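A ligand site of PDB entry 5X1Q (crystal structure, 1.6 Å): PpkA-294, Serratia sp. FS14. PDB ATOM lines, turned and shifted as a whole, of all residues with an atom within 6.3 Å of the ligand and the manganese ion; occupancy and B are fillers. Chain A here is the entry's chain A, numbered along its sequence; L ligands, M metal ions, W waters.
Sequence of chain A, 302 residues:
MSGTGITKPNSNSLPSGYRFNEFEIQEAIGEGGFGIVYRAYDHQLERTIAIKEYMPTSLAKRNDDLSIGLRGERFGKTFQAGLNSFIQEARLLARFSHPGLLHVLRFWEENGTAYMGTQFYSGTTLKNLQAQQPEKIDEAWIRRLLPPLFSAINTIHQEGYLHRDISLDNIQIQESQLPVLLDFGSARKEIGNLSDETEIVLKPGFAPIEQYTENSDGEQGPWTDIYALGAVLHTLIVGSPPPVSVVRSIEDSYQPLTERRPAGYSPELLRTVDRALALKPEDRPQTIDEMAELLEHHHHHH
O of Ser 122 lies within hydrogen-bond range of NE2 of Gln 172, at 3.0 Å.
N of Ile 29 is in hydrogen-bond range of O of Val 37, 2.8 Å away.
The side-chain amide nitrogen of Gln 172 sits at hydrogen-bond distance from the backbone carbonyl oxygen of Gly 123, 3.3 Å away.
The backbone carbonyl oxygen (O) of Gly 30 is in hydrogen-bond range of the backbone NH (N) of Val 37, 2.8 Å away.
NZ of Lys 52 is in hydrogen-bond range of O of Leu 182, at 3.2 Å.
The side-chain amide oxygen (OD1) of Asn 128 is in hydrogen-bond range of the side-chain amino group (NZ) of Lys 127 (3.0 Å).
ND2 of Asn 128 is in hydrogen-bond range of OG1 of Thr 124, 3.1 Å away.
N of Asn 128 sits at hydrogen-bond distance from OG1 of Thr 125, 3.1 Å away.
The manganese ion is bound by O5 of the ligand (2.3 Å), O3 of the ligand (2.3 Å), water W4 (2.5 Å) and water W2 (2.6 Å).
No residue comes within 4 Å of the manganese ion.
Water W2 bridges OD1 of Asn 128 and O2 of the ligand.
Water W6 lies within hydrogen-bond range of OG1 of Thr 125 (2.5 Å), O2 of the ligand (2.7 Å) and ND2 of Asn 128 (3.2 Å).
Water W8 lies within hydrogen-bond range of an oxygen (O12) of the ligand (2.7 Å) and the side-chain hydroxyl of Thr 124 (3.0 Å).
Water W3 lies within hydrogen-bond range of the side-chain amino group (NZ) of Lys 52 (3.0 Å), a nitrogen (N2) of the ligand (3.0 Å) and the backbone carbonyl oxygen (O) of Leu 182 (3.2 Å).
Water W5 lies within hydrogen-bond range of the backbone carbonyl oxygen of Ile 29 and an oxygen (O12) of the ligand.
Water W1 lies within hydrogen-bond range of OD1 of Asp 169 (2.6 Å) and O8 of the ligand (3.0 Å).
The side-chain amide nitrogen (ND2) of Asn 128 sits at hydrogen-bond distance from an oxygen (O2) of the ligand, at 2.9 Å.
OG1 of Thr 118 lies within hydrogen-bond range of N3 of the ligand, at 3.4 Å.
The side-chain amide oxygen (OE1) of Gln 172 lies within hydrogen-bond range of an oxygen (O13) of the ligand.
N of Glu 31 sits at hydrogen-bond distance from O4 of the ligand, 3.1 Å away.
The backbone NH (N) of Tyr 121 lies within hydrogen-bond range of a nitrogen (N4) of the ligand, 3.0 Å away.
A nitrogen (N3) of the ligand sits at hydrogen-bond distance from the backbone carbonyl oxygen of Gln 119.
CD1 of Ile 29 touches N5 of the ligand, at 3.5 Å.
Gly 30 touches the ligand.
Gly 32 touches the ligand (N to O7, 3.7 Å).
Val 37 touches the ligand.
Ala 50 touches the ligand (CB to N3, 3.6 Å).
Leu 102 touches the ligand.
Phe 120 touches the ligand.
Thr 125 touches the ligand (CG2 to O13, 3.5 Å).
CD2 of Leu 182 touches N2 of the ligand, at 3.9 Å.
Hydrophobic or aromatic side chains within 4 Å of the ligand: Ile 29, Val 37, Ala 50, Leu 102, Phe 120, Tyr 121 and Leu 182.
Within 4 Å of the ligand: Ile 29, Gly 30, Glu 31, Gly 32, Val 37, Ala 50, Leu 102, Thr 118, Gln 119, Phe 120, Tyr 121, Thr 125, Asn 128, Gln 172 and Leu 182.
Along chain A the residues within 4 Å of the ligand span positions 29 to 182.
The nearest printed residue that does not touch the ligand is Thr 124 (4.3 Å).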
ATOM      1  N   ILE A  29       0.011  26.064 -27.086  1.00  0.00           N
ATOM      2  CA  ILE A  29      -1.013  26.949 -27.626  1.00  0.00           C
ATOM      3  C   ILE A  29      -1.811  27.624 -26.531  1.00  0.00           C
ATOM      4  O   ILE A  29      -2.565  28.561 -26.838  1.00  0.00           O
ATOM      5  CB  ILE A  29      -1.952  26.203 -28.592  1.00  0.00           C
ATOM      6  CG1 ILE A  29      -2.682  25.073 -27.867  1.00  0.00           C
ATOM      7  CG2 ILE A  29      -1.129  25.666 -29.768  1.00  0.00           C
ATOM      8  CD1 ILE A  29      -3.783  24.401 -28.715  1.00  0.00           C
ATOM      9  N   GLY A  30      -1.704  27.163 -25.294  1.00  0.00           N
ATOM     10  CA  GLY A  30      -2.299  27.880 -24.192  1.00  0.00           C
ATOM     11  C   GLY A  30      -1.403  27.770 -22.982  1.00  0.00           C
ATOM     12  O   GLY A  30      -0.881  26.701 -22.682  1.00  0.00           O
ATOM     13  N   GLU A  31      -1.182  28.890 -22.288  1.00  0.00           N
ATOM     14  CA  GLU A  31      -0.403  28.852 -21.063  1.00  0.00           C
ATOM     15  C   GLU A  31      -1.085  29.777 -20.067  1.00  0.00           C
ATOM     16  O   GLU A  31      -1.089  30.991 -20.253  1.00  0.00           O
ATOM     17  CB  GLU A  31       1.043  29.277 -21.281  1.00  0.00           C
ATOM     18  CG  GLU A  31       1.882  29.144 -20.019  1.00  0.00           C
ATOM     19  CD  GLU A  31       3.360  28.984 -20.318  1.00  0.00           C
ATOM     20  OE1 GLU A  31       3.780  29.310 -21.443  1.00  0.00           O
ATOM     21  OE2 GLU A  31       4.096  28.519 -19.411  1.00  0.00           O
ATOM     22  N   GLY A  32      -1.681  29.185 -19.042  1.00  0.00           N
ATOM     23  CA  GLY A  32      -2.355  29.954 -18.029  1.00  0.00           C
ATOM     24  C   GLY A  32      -1.719  29.717 -16.677  1.00  0.00           C
ATOM     25  O   GLY A  32      -0.671  29.059 -16.576  1.00  0.00           O
ATOM     26  N   GLY A  33      -2.343  30.252 -15.632  1.00  0.00           N
ATOM     27  CA  GLY A  33      -1.804  30.084 -14.313  1.00  0.00           C
ATOM     28  C   GLY A  33      -1.873  28.676 -13.783  1.00  0.00           C
ATOM     29  O   GLY A  33      -1.211  28.380 -12.782  1.00  0.00           O
ATOM     30  N   GLY A  35      -2.501  25.531 -16.025  1.00  0.00           N
ATOM     31  CA  GLY A  35      -2.179  24.451 -16.922  1.00  0.00           C
ATOM     32  C   GLY A  35      -1.653  24.990 -18.234  1.00  0.00           C
ATOM     33  O   GLY A  35      -1.814  26.167 -18.554  1.00  0.00           O
ATOM     34  N   VAL A  37      -1.650  24.037 -22.458  1.00  0.00           N
ATOM     35  CA  VAL A  37      -2.259  23.251 -23.516  1.00  0.00           C
ATOM     36  C   VAL A  37      -1.302  23.214 -24.690  1.00  0.00           C
ATOM     37  O   VAL A  37      -0.833  24.272 -25.140  1.00  0.00           O
ATOM     38  CB  VAL A  37      -3.614  23.833 -23.951  1.00  0.00           C
ATOM     39  CG1 VAL A  37      -4.221  22.940 -25.038  1.00  0.00           C
ATOM     40  CG2 VAL A  37      -4.542  23.974 -22.739  1.00  0.00           C
ATOM     41  N   ALA A  50      -4.672  17.397 -28.680  1.00  0.00           N
ATOM     42  CA  ALA A  50      -4.217  18.360 -27.686  1.00  0.00           C
ATOM     43  C   ALA A  50      -3.747  17.591 -26.452  1.00  0.00           C
ATOM     44  O   ALA A  50      -4.251  16.516 -26.151  1.00  0.00           O
ATOM     45  CB  ALA A  50      -5.310  19.351 -27.286  1.00  0.00           C
ATOM     46  N   LYS A  52      -3.191  18.499 -22.365  1.00  0.00           N
ATOM     47  CA  LYS A  52      -3.368  19.442 -21.267  1.00  0.00           C
ATOM     48  C   LYS A  52      -2.474  18.987 -20.123  1.00  0.00           C
ATOM     49  O   LYS A  52      -2.584  17.841 -19.669  1.00  0.00           O
ATOM     50  CB  LYS A  52      -4.820  19.512 -20.795  1.00  0.00           C
ATOM     51  CG  LYS A  52      -5.801  19.919 -21.870  1.00  0.00           C
ATOM     52  CD  LYS A  52      -7.246  19.917 -21.351  1.00  0.00           C
ATOM     53  CE  LYS A  52      -7.463  20.920 -20.211  1.00  0.00           C
ATOM     54  NZ  LYS A  52      -8.939  21.136 -19.994  1.00  0.00           N
ATOM     55  N   LEU A 102     -15.467  18.625 -24.495  1.00  0.00           N
ATOM     56  CA  LEU A 102     -14.087  18.220 -24.760  1.00  0.00           C
ATOM     57  C   LEU A 102     -13.938  16.716 -24.652  1.00  0.00           C
ATOM     58  O   LEU A 102     -14.246  16.132 -23.605  1.00  0.00           O
ATOM     59  CB  LEU A 102     -13.171  18.912 -23.741  1.00  0.00           C
ATOM     60  CG  LEU A 102     -11.671  18.533 -23.751  1.00  0.00           C
ATOM     61  CD1 LEU A 102     -10.896  19.512 -24.564  1.00  0.00           C
ATOM     62  CD2 LEU A 102     -11.164  18.516 -22.319  1.00  0.00           C
ATOM     63  N   THR A 118      -6.449  14.871 -25.487  1.00  0.00           N
ATOM     64  CA  THR A 118      -7.823  15.175 -25.886  1.00  0.00           C
ATOM     65  C   THR A 118      -7.893  15.421 -27.387  1.00  0.00           C
ATOM     66  O   THR A 118      -6.885  15.574 -28.072  1.00  0.00           O
ATOM     67  CB  THR A 118      -8.403  16.410 -25.159  1.00  0.00           C
ATOM     68  OG1 THR A 118      -7.887  17.606 -25.763  1.00  0.00           O
ATOM     69  CG2 THR A 118      -8.044  16.396 -23.685  1.00  0.00           C
ATOM     70  N   GLN A 119      -9.127  15.431 -27.886  1.00  0.00           N
ATOM     71  CA  GLN A 119      -9.347  15.857 -29.247  1.00  0.00           C
ATOM     72  C   GLN A 119      -8.806  17.274 -29.429  1.00  0.00           C
ATOM     73  O   GLN A 119      -8.872  18.092 -28.516  1.00  0.00           O
ATOM     74  CB  GLN A 119     -10.844  15.806 -29.555  1.00  0.00           C
ATOM     75  CG  GLN A 119     -11.219  16.172 -30.972  1.00  0.00           C
ATOM     76  CD  GLN A 119     -12.615  15.708 -31.299  1.00  0.00           C
ATOM     77  OE1 GLN A 119     -13.107  14.745 -30.708  1.00  0.00           O
ATOM     78  NE2 GLN A 119     -13.255  16.397 -32.231  1.00  0.00           N
ATOM     79  N   PHE A 120      -8.274  17.550 -30.616  1.00  0.00           N
ATOM     80  CA  PHE A 120      -7.802  18.880 -30.966  1.00  0.00           C
ATOM     81  C   PHE A 120      -8.882  19.594 -31.757  1.00  0.00           C
ATOM     82  O   PHE A 120      -9.368  19.067 -32.759  1.00  0.00           O
ATOM     83  CB  PHE A 120      -6.496  18.810 -31.768  1.00  0.00           C
ATOM     84  CG  PHE A 120      -5.966  20.154 -32.155  1.00  0.00           C
ATOM     85  CD1 PHE A 120      -5.198  20.895 -31.285  1.00  0.00           C
ATOM     86  CD2 PHE A 120      -6.264  20.689 -33.395  1.00  0.00           C
ATOM     87  CE1 PHE A 120      -4.738  22.154 -31.650  1.00  0.00           C
ATOM     88  CE2 PHE A 120      -5.795  21.945 -33.756  1.00  0.00           C
ATOM     89  CZ  PHE A 120      -5.026  22.661 -32.886  1.00  0.00           C
ATOM     90  N   TYR A 121      -9.267  20.783 -31.299  1.00  0.00           N
ATOM     91  CA  TYR A 121     -10.326  21.550 -31.929  1.00  0.00           C
ATOM     92  C   TYR A 121      -9.781  22.728 -32.721  1.00  0.00           C
ATOM     93  O   TYR A 121      -8.840  23.396 -32.284  1.00  0.00           O
ATOM     94  CB  TYR A 121     -11.347  22.061 -30.891  1.00  0.00           C
ATOM     95  CG  TYR A 121     -11.979  20.910 -30.167  1.00  0.00           C
ATOM     96  CD1 TYR A 121     -13.025  20.187 -30.739  1.00  0.00           C
ATOM     97  CD2 TYR A 121     -11.502  20.509 -28.935  1.00  0.00           C
ATOM     98  CE1 TYR A 121     -13.585  19.104 -30.086  1.00  0.00           C
ATOM     99  CE2 TYR A 121     -12.043  19.431 -28.267  1.00  0.00           C
ATOM    100  CZ  TYR A 121     -13.077  18.721 -28.854  1.00  0.00           C
ATOM    101  OH  TYR A 121     -13.624  17.642 -28.199  1.00  0.00           O
ATOM    102  N   SER A 122     -10.401  22.961 -33.875  1.00  0.00           N
ATOM    103  CA  SER A 122     -10.113  24.145 -34.665  1.00  0.00           C
ATOM    104  C   SER A 122     -10.670  25.388 -33.982  1.00  0.00           C
ATOM    105  O   SER A 122     -11.358  25.315 -32.962  1.00  0.00           O
ATOM    106  CB  SER A 122     -10.718  24.003 -36.059  1.00  0.00           C
ATOM    107  OG  SER A 122     -12.129  24.028 -35.985  1.00  0.00           O
ATOM    108  N   GLY A 123     -10.368  26.548 -34.564  1.00  0.00           N
ATOM    109  CA  GLY A 123     -10.913  27.796 -34.061  1.00  0.00           C
ATOM    110  C   GLY A 123     -10.146  28.334 -32.859  1.00  0.00           C
ATOM    111  O   GLY A 123      -8.968  28.055 -32.655  1.00  0.00           O
ATOM    112  N   THR A 124     -10.860  29.119 -32.055  1.00  0.00           N
ATOM    113  CA  THR A 124     -10.288  29.743 -30.862  1.00  0.00           C
ATOM    114  C   THR A 124     -11.417  29.929 -29.868  1.00  0.00           C
ATOM    115  O   THR A 124     -12.555  29.522 -30.113  1.00  0.00           O
ATOM    116  CB  THR A 124      -9.595  31.065 -31.211  1.00  0.00           C
ATOM    117  OG1 THR A 124      -8.825  31.504 -30.086  1.00  0.00           O
ATOM    118  CG2 THR A 124     -10.609  32.116 -31.589  1.00  0.00           C
ATOM    119  N   THR A 125     -11.101  30.521 -28.711  1.00  0.00           N
ATOM    120  CA  THR A 125     -12.098  30.706 -27.672  1.00  0.00           C
ATOM    121  C   THR A 125     -13.099  31.786 -28.050  1.00  0.00           C
ATOM    122  O   THR A 125     -12.814  32.679 -28.851  1.00  0.00           O
ATOM    123  CB  THR A 125     -11.459  31.085 -26.337  1.00  0.00           C
ATOM    124  OG1 THR A 125     -10.736  32.314 -26.476  1.00  0.00           O
ATOM    125  CG2 THR A 125     -10.542  29.983 -25.845  1.00  0.00           C
ATOM    126  N   LYS A 127     -13.905  34.082 -26.054  1.00  0.00           N
ATOM    127  CA  LYS A 127     -13.282  35.301 -25.557  1.00  0.00           C
ATOM    128  C   LYS A 127     -12.413  35.945 -26.642  1.00  0.00           C
ATOM    129  O   LYS A 127     -12.493  37.151 -26.876  1.00  0.00           O
ATOM    130  CB  LYS A 127     -12.458  34.997 -24.297  1.00  0.00           C
ATOM    131  CG  LYS A 127     -11.905  36.241 -23.592  1.00  0.00           C
ATOM    132  CD  LYS A 127     -10.819  35.873 -22.611  1.00  0.00           C
ATOM    133  CE  LYS A 127      -9.748  35.077 -23.299  1.00  0.00           C
ATOM    134  NZ  LYS A 127      -8.762  35.960 -23.993  1.00  0.00           N
ATOM    135  N   ASN A 128     -11.616  35.136 -27.335  1.00  0.00           N
ATOM    136  CA  ASN A 128     -10.754  35.703 -28.374  1.00  0.00           C
ATOM    137  C   ASN A 128     -11.572  36.168 -29.572  1.00  0.00           C
ATOM    138  O   ASN A 128     -11.245  37.197 -30.178  1.00  0.00           O
ATOM    139  CB  ASN A 128      -9.690  34.693 -28.806  1.00  0.00           C
ATOM    140  CG  ASN A 128      -8.624  34.494 -27.751  1.00  0.00           C
ATOM    141  OD1 ASN A 128      -8.428  35.342 -26.868  1.00  0.00           O
ATOM    142  ND2 ASN A 128      -7.921  33.385 -27.840  1.00  0.00           N
ATOM    143  N   ASP A 169     -14.240  32.372 -21.636  1.00  0.00           N
ATOM    144  CA  ASP A 169     -12.857  31.930 -21.679  1.00  0.00           C
ATOM    145  C   ASP A 169     -12.719  30.443 -21.978  1.00  0.00           C
ATOM    146  O   ASP A 169     -11.680  30.020 -22.498  1.00  0.00           O
ATOM    147  CB  ASP A 169     -12.246  32.342 -20.331  1.00  0.00           C
ATOM    148  CG  ASP A 169     -10.837  31.929 -20.167  1.00  0.00           C
ATOM    149  OD1 ASP A 169      -9.949  32.490 -20.846  1.00  0.00           O
ATOM    150  OD2 ASP A 169     -10.606  31.087 -19.286  1.00  0.00           O
ATOM    151  N   GLN A 172     -14.844  26.975 -26.719  1.00  0.00           N
ATOM    152  CA  GLN A 172     -14.174  27.030 -28.006  1.00  0.00           C
ATOM    153  C   GLN A 172     -15.196  27.239 -29.100  1.00  0.00           C
ATOM    154  O   GLN A 172     -16.269  26.631 -29.077  1.00  0.00           O
ATOM    155  CB  GLN A 172     -13.411  25.725 -28.260  1.00  0.00           C
ATOM    156  CG  GLN A 172     -12.540  25.695 -29.526  1.00  0.00           C
ATOM    157  CD  GLN A 172     -11.166  26.259 -29.263  1.00  0.00           C
ATOM    158  OE1 GLN A 172     -10.897  26.791 -28.191  1.00  0.00           O
ATOM    159  NE2 GLN A 172     -10.274  26.149 -30.260  1.00  0.00           N
ATOM    160  N   LEU A 182     -14.593  23.411 -22.928  1.00  0.00           N
ATOM    161  CA  LEU A 182     -13.200  22.951 -22.825  1.00  0.00           C
ATOM    162  C   LEU A 182     -12.762  22.539 -21.439  1.00  0.00           C
ATOM    163  O   LEU A 182     -11.803  21.764 -21.305  1.00  0.00           O
ATOM    164  CB  LEU A 182     -12.248  24.050 -23.288  1.00  0.00           C
ATOM    165  CG  LEU A 182     -12.322  24.468 -24.747  1.00  0.00           C
ATOM    166  CD1 LEU A 182     -11.459  25.718 -24.941  1.00  0.00           C
ATOM    167  CD2 LEU A 182     -11.868  23.339 -25.668  1.00  0.00           C
HETATM  168  P1  LIG L   1      -4.960  32.553 -25.810  1.00  0.00           P
HETATM  169  O1  LIG L   1      -4.247  32.519 -27.147  1.00  0.00           O
HETATM  170  O2  LIG L   1      -6.370  32.003 -25.874  1.00  0.00           O
HETATM  171  O3  LIG L   1      -4.835  33.874 -25.076  1.00  0.00           O
HETATM  172  P2  LIG L   1      -3.422  31.645 -23.516  1.00  0.00           P
HETATM  173  O4  LIG L   1      -1.940  31.461 -23.769  1.00  0.00           O
HETATM  174  O5  LIG L   1      -3.919  32.851 -22.766  1.00  0.00           O
HETATM  175  O6  LIG L   1      -4.205  31.434 -24.920  1.00  0.00           O
HETATM  176  P3  LIG L   1      -5.235  30.060 -21.915  1.00  0.00           P
HETATM  177  O7  LIG L   1      -4.853  28.993 -20.904  1.00  0.00           O
HETATM  178  O8  LIG L   1      -5.845  31.350 -21.436  1.00  0.00           O
HETATM  179  O9  LIG L   1      -3.883  30.298 -22.760  1.00  0.00           O
HETATM  180  O10 LIG L   1      -6.194  29.430 -23.042  1.00  0.00           O
HETATM  181  C1  LIG L   1      -6.163  28.044 -23.369  1.00  0.00           C
HETATM  182  C2  LIG L   1      -5.978  27.986 -24.868  1.00  0.00           C
HETATM  183  O11 LIG L   1      -5.934  26.624 -25.283  1.00  0.00           O
HETATM  184  C3  LIG L   1      -7.116  28.645 -25.636  1.00  0.00           C
HETATM  185  O12 LIG L   1      -6.560  29.427 -26.704  1.00  0.00           O
HETATM  186  C4  LIG L   1      -7.886  27.488 -26.244  1.00  0.00           C
HETATM  187  O13 LIG L   1      -8.440  27.774 -27.520  1.00  0.00           O
HETATM  188  C5  LIG L   1      -6.813  26.426 -26.378  1.00  0.00           C
HETATM  189  N1  LIG L   1      -7.310  25.030 -26.274  1.00  0.00           N
HETATM  190  C6  LIG L   1      -7.622  24.411 -25.122  1.00  0.00           C
HETATM  191  N2  LIG L   1      -8.021  23.136 -25.357  1.00  0.00           N
HETATM  192  C7  LIG L   1      -7.945  22.946 -26.685  1.00  0.00           C
HETATM  193  C8  LIG L   1      -8.196  21.809 -27.593  1.00  0.00           C
HETATM  194  N3  LIG L   1      -8.622  20.635 -27.091  1.00  0.00           N
HETATM  195  N4  LIG L   1      -7.993  22.004 -28.913  1.00  0.00           N
HETATM  196  C9  LIG L   1      -7.564  23.190 -29.410  1.00  0.00           C
HETATM  197  N5  LIG L   1      -7.303  24.264 -28.639  1.00  0.00           N
HETATM  198  C10 LIG L   1      -7.466  24.186 -27.296  1.00  0.00           C
HETATM  199 MN    MN M   1      -4.395  35.093 -23.142  1.00  0.00          MN
HETATM  200  O   HOH W   1      -8.640  31.191 -22.610  1.00  0.00           O
HETATM  201  O   HOH W   2      -6.684  34.847 -24.344  1.00  0.00           O
HETATM  202  O   HOH W   3      -8.994  22.537 -22.599  1.00  0.00           O
HETATM  203  O   HOH W   4      -5.150  37.494 -23.083  1.00  0.00           O
HETATM  204  O   HOH W   5      -4.323  29.184 -28.702  1.00  0.00           O
HETATM  205  O   HOH W   6      -8.780  32.545 -24.885  1.00  0.00           O
HETATM  206  O   HOH W   7      -3.802  26.685 -20.560  1.00  0.00           O
HETATM  207  O   HOH W   8      -6.998  29.172 -29.395  1.00  0.00           O
